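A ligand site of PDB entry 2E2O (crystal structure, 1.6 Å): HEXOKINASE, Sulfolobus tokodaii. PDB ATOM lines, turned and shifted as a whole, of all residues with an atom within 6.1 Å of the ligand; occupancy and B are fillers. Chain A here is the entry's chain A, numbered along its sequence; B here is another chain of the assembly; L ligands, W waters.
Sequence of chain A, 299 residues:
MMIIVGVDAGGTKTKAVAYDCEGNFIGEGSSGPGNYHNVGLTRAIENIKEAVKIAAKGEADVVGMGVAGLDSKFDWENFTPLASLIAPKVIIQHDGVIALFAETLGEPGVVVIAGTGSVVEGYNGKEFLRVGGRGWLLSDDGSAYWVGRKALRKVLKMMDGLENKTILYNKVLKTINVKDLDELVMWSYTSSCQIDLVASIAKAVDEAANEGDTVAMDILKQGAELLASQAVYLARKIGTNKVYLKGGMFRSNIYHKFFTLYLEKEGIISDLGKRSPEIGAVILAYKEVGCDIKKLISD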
ATOM      1  N   GLY A  10      20.555  23.708  22.118  1.00  0.00           N
ATOM      2  CA  GLY A  10      20.068  22.462  22.666  1.00  0.00           C
ATOM      3  C   GLY A  10      20.095  21.237  21.774  1.00  0.00           C
ATOM      4  O   GLY A  10      20.605  21.262  20.652  1.00  0.00           O
ATOM      5  N   GLY A  11      19.538  20.147  22.294  1.00  0.00           N
ATOM      6  CA  GLY A  11      19.507  18.901  21.548  1.00  0.00           C
ATOM      7  C   GLY A  11      18.495  18.902  20.427  1.00  0.00           C
ATOM      8  O   GLY A  11      18.692  18.254  19.401  1.00  0.00           O
ATOM      9  N   ASN A  35      23.921  20.421  20.233  1.00  0.00           N
ATOM     10  CA  ASN A  35      24.574  19.355  20.979  1.00  0.00           C
ATOM     11  C   ASN A  35      25.481  18.586  20.009  1.00  0.00           C
ATOM     12  O   ASN A  35      24.998  17.829  19.174  1.00  0.00           O
ATOM     13  CB  ASN A  35      23.530  18.405  21.575  1.00  0.00           C
ATOM     14  CG  ASN A  35      24.151  17.381  22.504  1.00  0.00           C
ATOM     15  OD1 ASN A  35      25.317  17.031  22.371  1.00  0.00           O
ATOM     16  ND2 ASN A  35      23.359  16.877  23.453  1.00  0.00           N
ATOM     17  N   HIS A  37      27.271  16.066  20.391  1.00  0.00           N
ATOM     18  CA  HIS A  37      27.255  14.616  20.528  1.00  0.00           C
ATOM     19  C   HIS A  37      26.254  14.032  19.534  1.00  0.00           C
ATOM     20  O   HIS A  37      26.384  12.881  19.122  1.00  0.00           O
ATOM     21  CB  HIS A  37      26.860  14.212  21.951  1.00  0.00           C
ATOM     22  CG  HIS A  37      27.888  14.535  22.981  1.00  0.00           C
ATOM     23  ND1 HIS A  37      29.161  13.992  22.954  1.00  0.00           N
ATOM     24  CD2 HIS A  37      27.853  15.348  24.061  1.00  0.00           C
ATOM     25  CE1 HIS A  37      29.856  14.466  23.968  1.00  0.00           C
ATOM     26  NE2 HIS A  37      29.085  15.293  24.652  1.00  0.00           N
ATOM     27  N   ASN A  38      25.271  14.839  19.157  1.00  0.00           N
ATOM     28  CA  ASN A  38      24.230  14.402  18.226  1.00  0.00           C
ATOM     29  C   ASN A  38      24.466  14.737  16.758  1.00  0.00           C
ATOM     30  O   ASN A  38      24.016  14.008  15.877  1.00  0.00           O
ATOM     31  CB  ASN A  38      22.877  14.971  18.659  1.00  0.00           C
ATOM     32  CG  ASN A  38      22.454  14.504  20.045  1.00  0.00           C
ATOM     33  OD1 ASN A  38      21.386  14.868  20.535  1.00  0.00           O
ATOM     34  ND2 ASN A  38      23.292  13.686  20.669  1.00  0.00           N
ATOM     35  N   VAL A  67      24.841  25.636  26.442  1.00  0.00           N
ATOM     36  CA  VAL A  67      25.036  24.512  25.529  1.00  0.00           C
ATOM     37  C   VAL A  67      24.753  23.129  26.092  1.00  0.00           C
ATOM     38  O   VAL A  67      25.248  22.763  27.157  1.00  0.00           O
ATOM     39  CB  VAL A  67      26.493  24.523  25.001  1.00  0.00           C
ATOM     40  CG1 VAL A  67      26.660  23.507  23.885  1.00  0.00           C
ATOM     41  CG2 VAL A  67      26.858  25.925  24.526  1.00  0.00           C
ATOM     42  N   ALA A  68      23.965  22.349  25.362  1.00  0.00           N
ATOM     43  CA  ALA A  68      23.660  20.982  25.762  1.00  0.00           C
ATOM     44  C   ALA A  68      24.820  20.103  25.284  1.00  0.00           C
ATOM     45  O   ALA A  68      25.354  20.304  24.194  1.00  0.00           O
ATOM     46  CB  ALA A  68      22.357  20.512  25.106  1.00  0.00           C
ATOM     47  N   GLY A  69      25.214  19.131  26.106  1.00  0.00           N
ATOM     48  CA  GLY A  69      26.290  18.251  25.689  1.00  0.00           C
ATOM     49  C   GLY A  69      27.659  18.489  26.313  1.00  0.00           C
ATOM     50  O   GLY A  69      28.564  17.683  26.112  1.00  0.00           O
ATOM     51  N   LEU A  70      27.819  19.594  27.035  1.00  0.00           N
ATOM     52  CA  LEU A  70      29.108  19.861  27.689  1.00  0.00           C
ATOM     53  C   LEU A  70      28.980  19.103  29.001  1.00  0.00           C
ATOM     54  O   LEU A  70      28.669  19.666  30.044  1.00  0.00           O
ATOM     55  CB  LEU A  70      29.271  21.363  27.933  1.00  0.00           C
ATOM     56  CG  LEU A  70      29.212  22.214  26.665  1.00  0.00           C
ATOM     57  CD1 LEU A  70      29.477  23.667  27.014  1.00  0.00           C
ATOM     58  CD2 LEU A  70      30.232  21.706  25.646  1.00  0.00           C
ATOM     59  N   ASP A  71      29.234  17.796  28.920  1.00  0.00           N
ATOM     60  CA  ASP A  71      29.081  16.885  30.044  1.00  0.00           C
ATOM     61  C   ASP A  71      30.344  16.330  30.678  1.00  0.00           C
ATOM     62  O   ASP A  71      30.269  15.516  31.609  1.00  0.00           O
ATOM     63  CB  ASP A  71      28.183  15.730  29.597  1.00  0.00           C
ATOM     64  CG  ASP A  71      26.855  16.217  29.027  1.00  0.00           C
ATOM     65  OD1 ASP A  71      26.191  15.443  28.300  1.00  0.00           O
ATOM     66  OD2 ASP A  71      26.481  17.373  29.321  1.00  0.00           O
ATOM     67  N   HIS A  94      27.028  25.671  30.433  1.00  0.00           N
ATOM     68  CA  HIS A  94      26.202  24.496  30.204  1.00  0.00           C
ATOM     69  C   HIS A  94      24.769  25.026  30.090  1.00  0.00           C
ATOM     70  O   HIS A  94      24.436  26.033  30.724  1.00  0.00           O
ATOM     71  CB  HIS A  94      26.330  23.547  31.404  1.00  0.00           C
ATOM     72  CG  HIS A  94      25.428  22.357  31.335  1.00  0.00           C
ATOM     73  ND1 HIS A  94      24.527  22.053  32.326  1.00  0.00           N
ATOM     74  CD2 HIS A  94      25.301  21.397  30.391  1.00  0.00           C
ATOM     75  CE1 HIS A  94      23.871  20.955  31.993  1.00  0.00           C
ATOM     76  NE2 HIS A  94      24.319  20.531  30.830  1.00  0.00           N
ATOM     77  N   ASP A  95      23.919  24.371  29.306  1.00  0.00           N
ATOM     78  CA  ASP A  95      22.562  24.890  29.160  1.00  0.00           C
ATOM     79  C   ASP A  95      21.742  24.948  30.446  1.00  0.00           C
ATOM     80  O   ASP A  95      20.925  25.851  30.610  1.00  0.00           O
ATOM     81  CB  ASP A  95      21.801  24.141  28.045  1.00  0.00           C
ATOM     82  CG  ASP A  95      21.596  22.663  28.320  1.00  0.00           C
ATOM     83  OD1 ASP A  95      22.242  22.104  29.234  1.00  0.00           O
ATOM     84  OD2 ASP A  95      20.794  22.056  27.588  1.00  0.00           O
ATOM     85  N   GLY A  96      21.983  24.008  31.357  1.00  0.00           N
ATOM     86  CA  GLY A  96      21.253  24.008  32.613  1.00  0.00           C
ATOM     87  C   GLY A  96      21.580  25.220  33.449  1.00  0.00           C
ATOM     88  O   GLY A  96      20.728  25.793  34.130  1.00  0.00           O
ATOM     89  N   ILE A 113      15.211  21.001  32.588  1.00  0.00           N
ATOM     90  CA  ILE A 113      15.152  21.166  31.148  1.00  0.00           C
ATOM     91  C   ILE A 113      14.712  19.800  30.653  1.00  0.00           C
ATOM     92  O   ILE A 113      15.354  18.783  30.956  1.00  0.00           O
ATOM     93  CB  ILE A 113      16.508  21.496  30.506  1.00  0.00           C
ATOM     94  CG1 ILE A 113      17.001  22.876  30.970  1.00  0.00           C
ATOM     95  CG2 ILE A 113      16.369  21.486  28.973  1.00  0.00           C
ATOM     96  CD1 ILE A 113      18.369  23.254  30.388  1.00  0.00           C
ATOM     97  N   ALA A 114      13.608  19.772  29.927  1.00  0.00           N
ATOM     98  CA  ALA A 114      13.115  18.523  29.355  1.00  0.00           C
ATOM     99  C   ALA A 114      12.868  18.765  27.876  1.00  0.00           C
ATOM    100  O   ALA A 114      11.845  19.332  27.509  1.00  0.00           O
ATOM    101  CB  ALA A 114      11.838  18.083  30.058  1.00  0.00           C
ATOM    102  N   GLY A 115      13.841  18.358  27.067  1.00  0.00           N
ATOM    103  CA  GLY A 115      13.748  18.512  25.622  1.00  0.00           C
ATOM    104  C   GLY A 115      14.167  17.207  24.974  1.00  0.00           C
ATOM    105  O   GLY A 115      13.656  16.153  25.327  1.00  0.00           O
ATOM    106  N   THR A 116      15.102  17.251  24.025  1.00  0.00           N
ATOM    107  CA  THR A 116      15.563  16.011  23.400  1.00  0.00           C
ATOM    108  C   THR A 116      16.272  15.197  24.476  1.00  0.00           C
ATOM    109  O   THR A 116      16.194  13.965  24.510  1.00  0.00           O
ATOM    110  CB  THR A 116      16.506  16.308  22.216  1.00  0.00           C
ATOM    111  OG1 THR A 116      15.717  16.709  21.090  1.00  0.00           O
ATOM    112  CG2 THR A 116      17.304  15.075  21.832  1.00  0.00           C
ATOM    113  N   GLY A 117      16.956  15.913  25.369  1.00  0.00           N
ATOM    114  CA  GLY A 117      17.630  15.300  26.498  1.00  0.00           C
ATOM    115  C   GLY A 117      17.036  16.007  27.714  1.00  0.00           C
ATOM    116  O   GLY A 117      16.139  16.839  27.552  1.00  0.00           O
ATOM    117  N   SER A 118      17.506  15.702  28.918  1.00  0.00           N
ATOM    118  CA  SER A 118      16.979  16.374  30.091  1.00  0.00           C
ATOM    119  C   SER A 118      18.052  16.576  31.147  1.00  0.00           C
ATOM    120  O   SER A 118      19.105  15.927  31.122  1.00  0.00           O
ATOM    121  CB  SER A 118      15.834  15.573  30.710  1.00  0.00           C
ATOM    122  OG  SER A 118      16.307  14.351  31.267  1.00  0.00           O
ATOM    123  N   VAL A 119      17.779  17.489  32.068  1.00  0.00           N
ATOM    124  CA  VAL A 119      18.713  17.766  33.155  1.00  0.00           C
ATOM    125  C   VAL A 119      18.033  18.566  34.248  1.00  0.00           C
ATOM    126  O   VAL A 119      17.032  19.260  34.007  1.00  0.00           O
ATOM    127  CB  VAL A 119      19.940  18.586  32.637  1.00  0.00           C
ATOM    128  CG1 VAL A 119      19.524  20.001  32.265  1.00  0.00           C
ATOM    129  CG2 VAL A 119      21.028  18.615  33.711  1.00  0.00           C
ATOM    130  N   ARG A 130      24.444  19.628  39.380  1.00  0.00           N
ATOM    131  CA  ARG A 130      23.710  18.972  38.294  1.00  0.00           C
ATOM    132  C   ARG A 130      23.293  17.550  38.665  1.00  0.00           C
ATOM    133  O   ARG A 130      24.016  16.836  39.345  1.00  0.00           O
ATOM    134  CB  ARG A 130      24.563  18.904  37.022  1.00  0.00           C
ATOM    135  CG  ARG A 130      23.770  18.494  35.789  1.00  0.00           C
ATOM    136  CD  ARG A 130      24.640  17.967  34.636  1.00  0.00           C
ATOM    137  NE  ARG A 130      25.693  18.898  34.232  1.00  0.00           N
ATOM    138  CZ  ARG A 130      26.308  18.857  33.054  1.00  0.00           C
ATOM    139  NH1 ARG A 130      25.977  17.943  32.144  1.00  0.00           N
ATOM    140  NH2 ARG A 130      27.269  19.725  32.785  1.00  0.00           N
ATOM    141  N   GLY A 133      21.405  14.717  33.042  1.00  0.00           N
ATOM    142  CA  GLY A 133      22.025  15.509  31.991  1.00  0.00           C
ATOM    143  C   GLY A 133      23.344  14.988  31.471  1.00  0.00           C
ATOM    144  O   GLY A 133      24.287  15.760  31.273  1.00  0.00           O
ATOM    145  N   ARG A 134      23.430  13.678  31.270  1.00  0.00           N
ATOM    146  CA  ARG A 134      24.657  13.068  30.759  1.00  0.00           C
ATOM    147  C   ARG A 134      24.413  12.196  29.531  1.00  0.00           C
ATOM    148  O   ARG A 134      25.073  11.172  29.353  1.00  0.00           O
ATOM    149  CB  ARG A 134      25.331  12.224  31.853  1.00  0.00           C
ATOM    150  CG  ARG A 134      25.568  12.962  33.167  1.00  0.00           C
ATOM    151  CD  ARG A 134      26.606  14.080  33.072  1.00  0.00           C
ATOM    152  NE  ARG A 134      26.732  14.764  34.358  1.00  0.00           N
ATOM    153  CZ  ARG A 134      27.622  15.710  34.648  1.00  0.00           C
ATOM    154  NH1 ARG A 134      28.498  16.115  33.737  1.00  0.00           N
ATOM    155  NH2 ARG A 134      27.630  16.250  35.856  1.00  0.00           N
ATOM    156  N   GLY A 135      23.456  12.571  28.683  1.00  0.00           N
ATOM    157  CA  GLY A 135      23.235  11.800  27.469  1.00  0.00           C
ATOM    158  C   GLY A 135      22.111  10.777  27.470  1.00  0.00           C
ATOM    159  O   GLY A 135      21.606  10.395  28.521  1.00  0.00           O
ATOM    160  N   TRP A 136      21.764  10.314  26.279  1.00  0.00           N
ATOM    161  CA  TRP A 136      20.667   9.364  26.104  1.00  0.00           C
ATOM    162  C   TRP A 136      20.839   7.971  26.698  1.00  0.00           C
ATOM    163  O   TRP A 136      19.866   7.381  27.163  1.00  0.00           O
ATOM    164  CB  TRP A 136      20.326   9.224  24.623  1.00  0.00           C
ATOM    165  CG  TRP A 136      21.448   8.682  23.794  1.00  0.00           C
ATOM    166  CD1 TRP A 136      22.450   9.401  23.207  1.00  0.00           C
ATOM    167  CD2 TRP A 136      21.703   7.302  23.484  1.00  0.00           C
ATOM    168  NE1 TRP A 136      23.318   8.552  22.548  1.00  0.00           N
ATOM    169  CE2 TRP A 136      22.888   7.262  22.707  1.00  0.00           C
ATOM    170  CE3 TRP A 136      21.049   6.099  23.788  1.00  0.00           C
ATOM    171  CZ2 TRP A 136      23.433   6.065  22.231  1.00  0.00           C
ATOM    172  CZ3 TRP A 136      21.595   4.902  23.312  1.00  0.00           C
ATOM    173  CH2 TRP A 136      22.768   4.901  22.548  1.00  0.00           C
ATOM    174  N   SER A 139      21.495   8.677  30.854  1.00  0.00           N
ATOM    175  CA  SER A 139      20.459   9.426  31.547  1.00  0.00           C
ATOM    176  C   SER A 139      19.306   9.908  30.672  1.00  0.00           C
ATOM    177  O   SER A 139      18.682   9.125  29.950  1.00  0.00           O
ATOM    178  CB  SER A 139      21.102  10.641  32.228  1.00  0.00           C
ATOM    179  OG  SER A 139      21.772  11.464  31.293  1.00  0.00           O
ATOM    180  N   ASP A 140      19.015  11.195  30.770  1.00  0.00           N
ATOM    181  CA  ASP A 140      17.923  11.828  30.047  1.00  0.00           C
ATOM    182  C   ASP A 140      16.535  11.230  30.324  1.00  0.00           C
ATOM    183  O   ASP A 140      15.729  11.052  29.411  1.00  0.00           O
ATOM    184  CB  ASP A 140      18.216  11.832  28.532  1.00  0.00           C
ATOM    185  CG  ASP A 140      19.340  12.807  28.172  1.00  0.00           C
ATOM    186  OD1 ASP A 140      19.730  13.591  29.052  1.00  0.00           O
ATOM    187  OD2 ASP A 140      19.817  12.789  27.012  1.00  0.00           O
ATOM    188  N   TYR B 189      30.082   7.936  25.781  1.00  0.00           N
ATOM    189  CA  TYR B 189      30.094   8.535  24.454  1.00  0.00           C
ATOM    190  C   TYR B 189      30.912   7.778  23.410  1.00  0.00           C
ATOM    191  O   TYR B 189      30.671   7.931  22.212  1.00  0.00           O
ATOM    192  CB  TYR B 189      30.540   9.998  24.547  1.00  0.00           C
ATOM    193  CG  TYR B 189      29.440  10.907  25.070  1.00  0.00           C
ATOM    194  CD1 TYR B 189      29.688  11.842  26.060  1.00  0.00           C
ATOM    195  CD2 TYR B 189      28.136  10.820  24.561  1.00  0.00           C
ATOM    196  CE1 TYR B 189      28.672  12.681  26.548  1.00  0.00           C
ATOM    197  CE2 TYR B 189      27.116  11.646  25.029  1.00  0.00           C
ATOM    198  CZ  TYR B 189      27.397  12.570  26.018  1.00  0.00           C
ATOM    199  OH  TYR B 189      26.393  13.391  26.486  1.00  0.00           O
HETATM  200  C1  LIG L   1      22.781  16.592  27.655  1.00  0.00           C
HETATM  201  C2  LIG L   1      22.917  17.656  28.763  1.00  0.00           C
HETATM  202  C3  LIG L   1      21.789  18.685  28.670  1.00  0.00           C
HETATM  203  C4  LIG L   1      20.437  17.978  28.619  1.00  0.00           C
HETATM  204  C5  LIG L   1      19.282  18.952  28.410  1.00  0.00           C
HETATM  205  C6  LIG L   1      21.374  16.008  27.663  1.00  0.00           C
HETATM  206  O1  LIG L   1      21.236  15.133  26.594  1.00  0.00           O
HETATM  207  O2  LIG L   1      23.719  15.555  27.877  1.00  0.00           O
HETATM  208  O3  LIG L   1      24.160  18.322  28.629  1.00  0.00           O
HETATM  209  O4  LIG L   1      21.844  19.528  29.808  1.00  0.00           O
HETATM  210  O5  LIG L   1      20.402  17.049  27.520  1.00  0.00           O
HETATM  211  O6  LIG L   1      19.481  19.749  27.248  1.00  0.00           O
HETATM  212  O   HOH W   1      20.634  16.394  24.161  1.00  0.00           O
HETATM  213  O   HOH W   2      18.739  18.294  24.792  1.00  0.00           O
HETATM  214  O   HOH W   3      24.160  14.525  25.198  1.00  0.00           O
HETATM  215  O   HOH W   4      17.916  21.276  25.215  1.00  0.00           O
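Water W1 lies within hydrogen-bond range of O1 of the ligand (2.8 Å) and ND2 of Asn 35 (2.9 Å). Water W3 lies within hydrogen-bond range of OH of Tyr 189 of chain B (2.8 Å), O2 of the ligand (2.9 Å) and ND2 of Asn 35 (3.0 Å). Water W2 lies within hydrogen-bond range of O6 of the ligand (2.9 Å), N of Gly 117 (3.0 Å) and N of Gly 11 (3.2 Å).
O1 of the ligand is in hydrogen-bond range of OD2 of Asp 140 (2.8 Å). OD1 of Asp 71 lies within hydrogen-bond range of O2 of the ligand (2.5 Å). An oxygen (O4) of the ligand lies within hydrogen-bond range of the side-chain carboxylate (OD1) of Asp 95 (2.7 Å). O3 of the ligand is in hydrogen-bond range of N of Gly 69 (2.9 Å). The backbone NH of Gly 135 is in hydrogen-bond range of an oxygen (O2) of the ligand. A ring nitrogen (NE2) of His 94 sits at hydrogen-bond distance from an oxygen (O4) of the ligand (2.9 Å). The backbone carbonyl oxygen of Gly 133 sits close to an oxygen (O2) of the ligand, at 3.4 Å. N of Ser 118 lies within hydrogen-bond range of O5 of the ligand (3.5 Å).
Merely in contact with the ligand: Ala 68 (3.7 Å), Ile 113 (3.9 Å), Gly 117 (3.4 Å), Val 119 (3.4 Å), Arg 130 (3.97 Å), Arg 134 (3.8 Å) and Tyr 189 of chain B (3.7 Å). Hydrophobic or aromatic side chains that line the ligand: Ala 68, His 94, Ile 113 and Val 119. The nearest printed residue that does not touch the ligand is Asn 35 (4.2 Å).
O of Asp 71 is in hydrogen-bond range of NH1 of Arg 134 (2.8 Å). The backbone NH (N) of Arg 134 is in hydrogen-bond range of the side-chain hydroxyl (OG) of Ser 139 (2.8 Å). OD1 of Asp 140 lies within hydrogen-bond range of N of Ser 118 (3.1 Å). ND1 of His 94 lies close to N of Gly 96 (3.4 Å). O of Val 67 lies within hydrogen-bond range of N of Asp 95 (3.0 Å). O of Val 119 is in hydrogen-bond range of N of Ile 113 (2.9 Å). A ring nitrogen (NE2) of His 94 sits at hydrogen-bond distance from the guanidinium group of Arg 130, 3.3 Å away. The side-chain carboxylate (OD2) of Asp 140 is in hydrogen-bond range of the backbone NH (N) of Trp 136.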
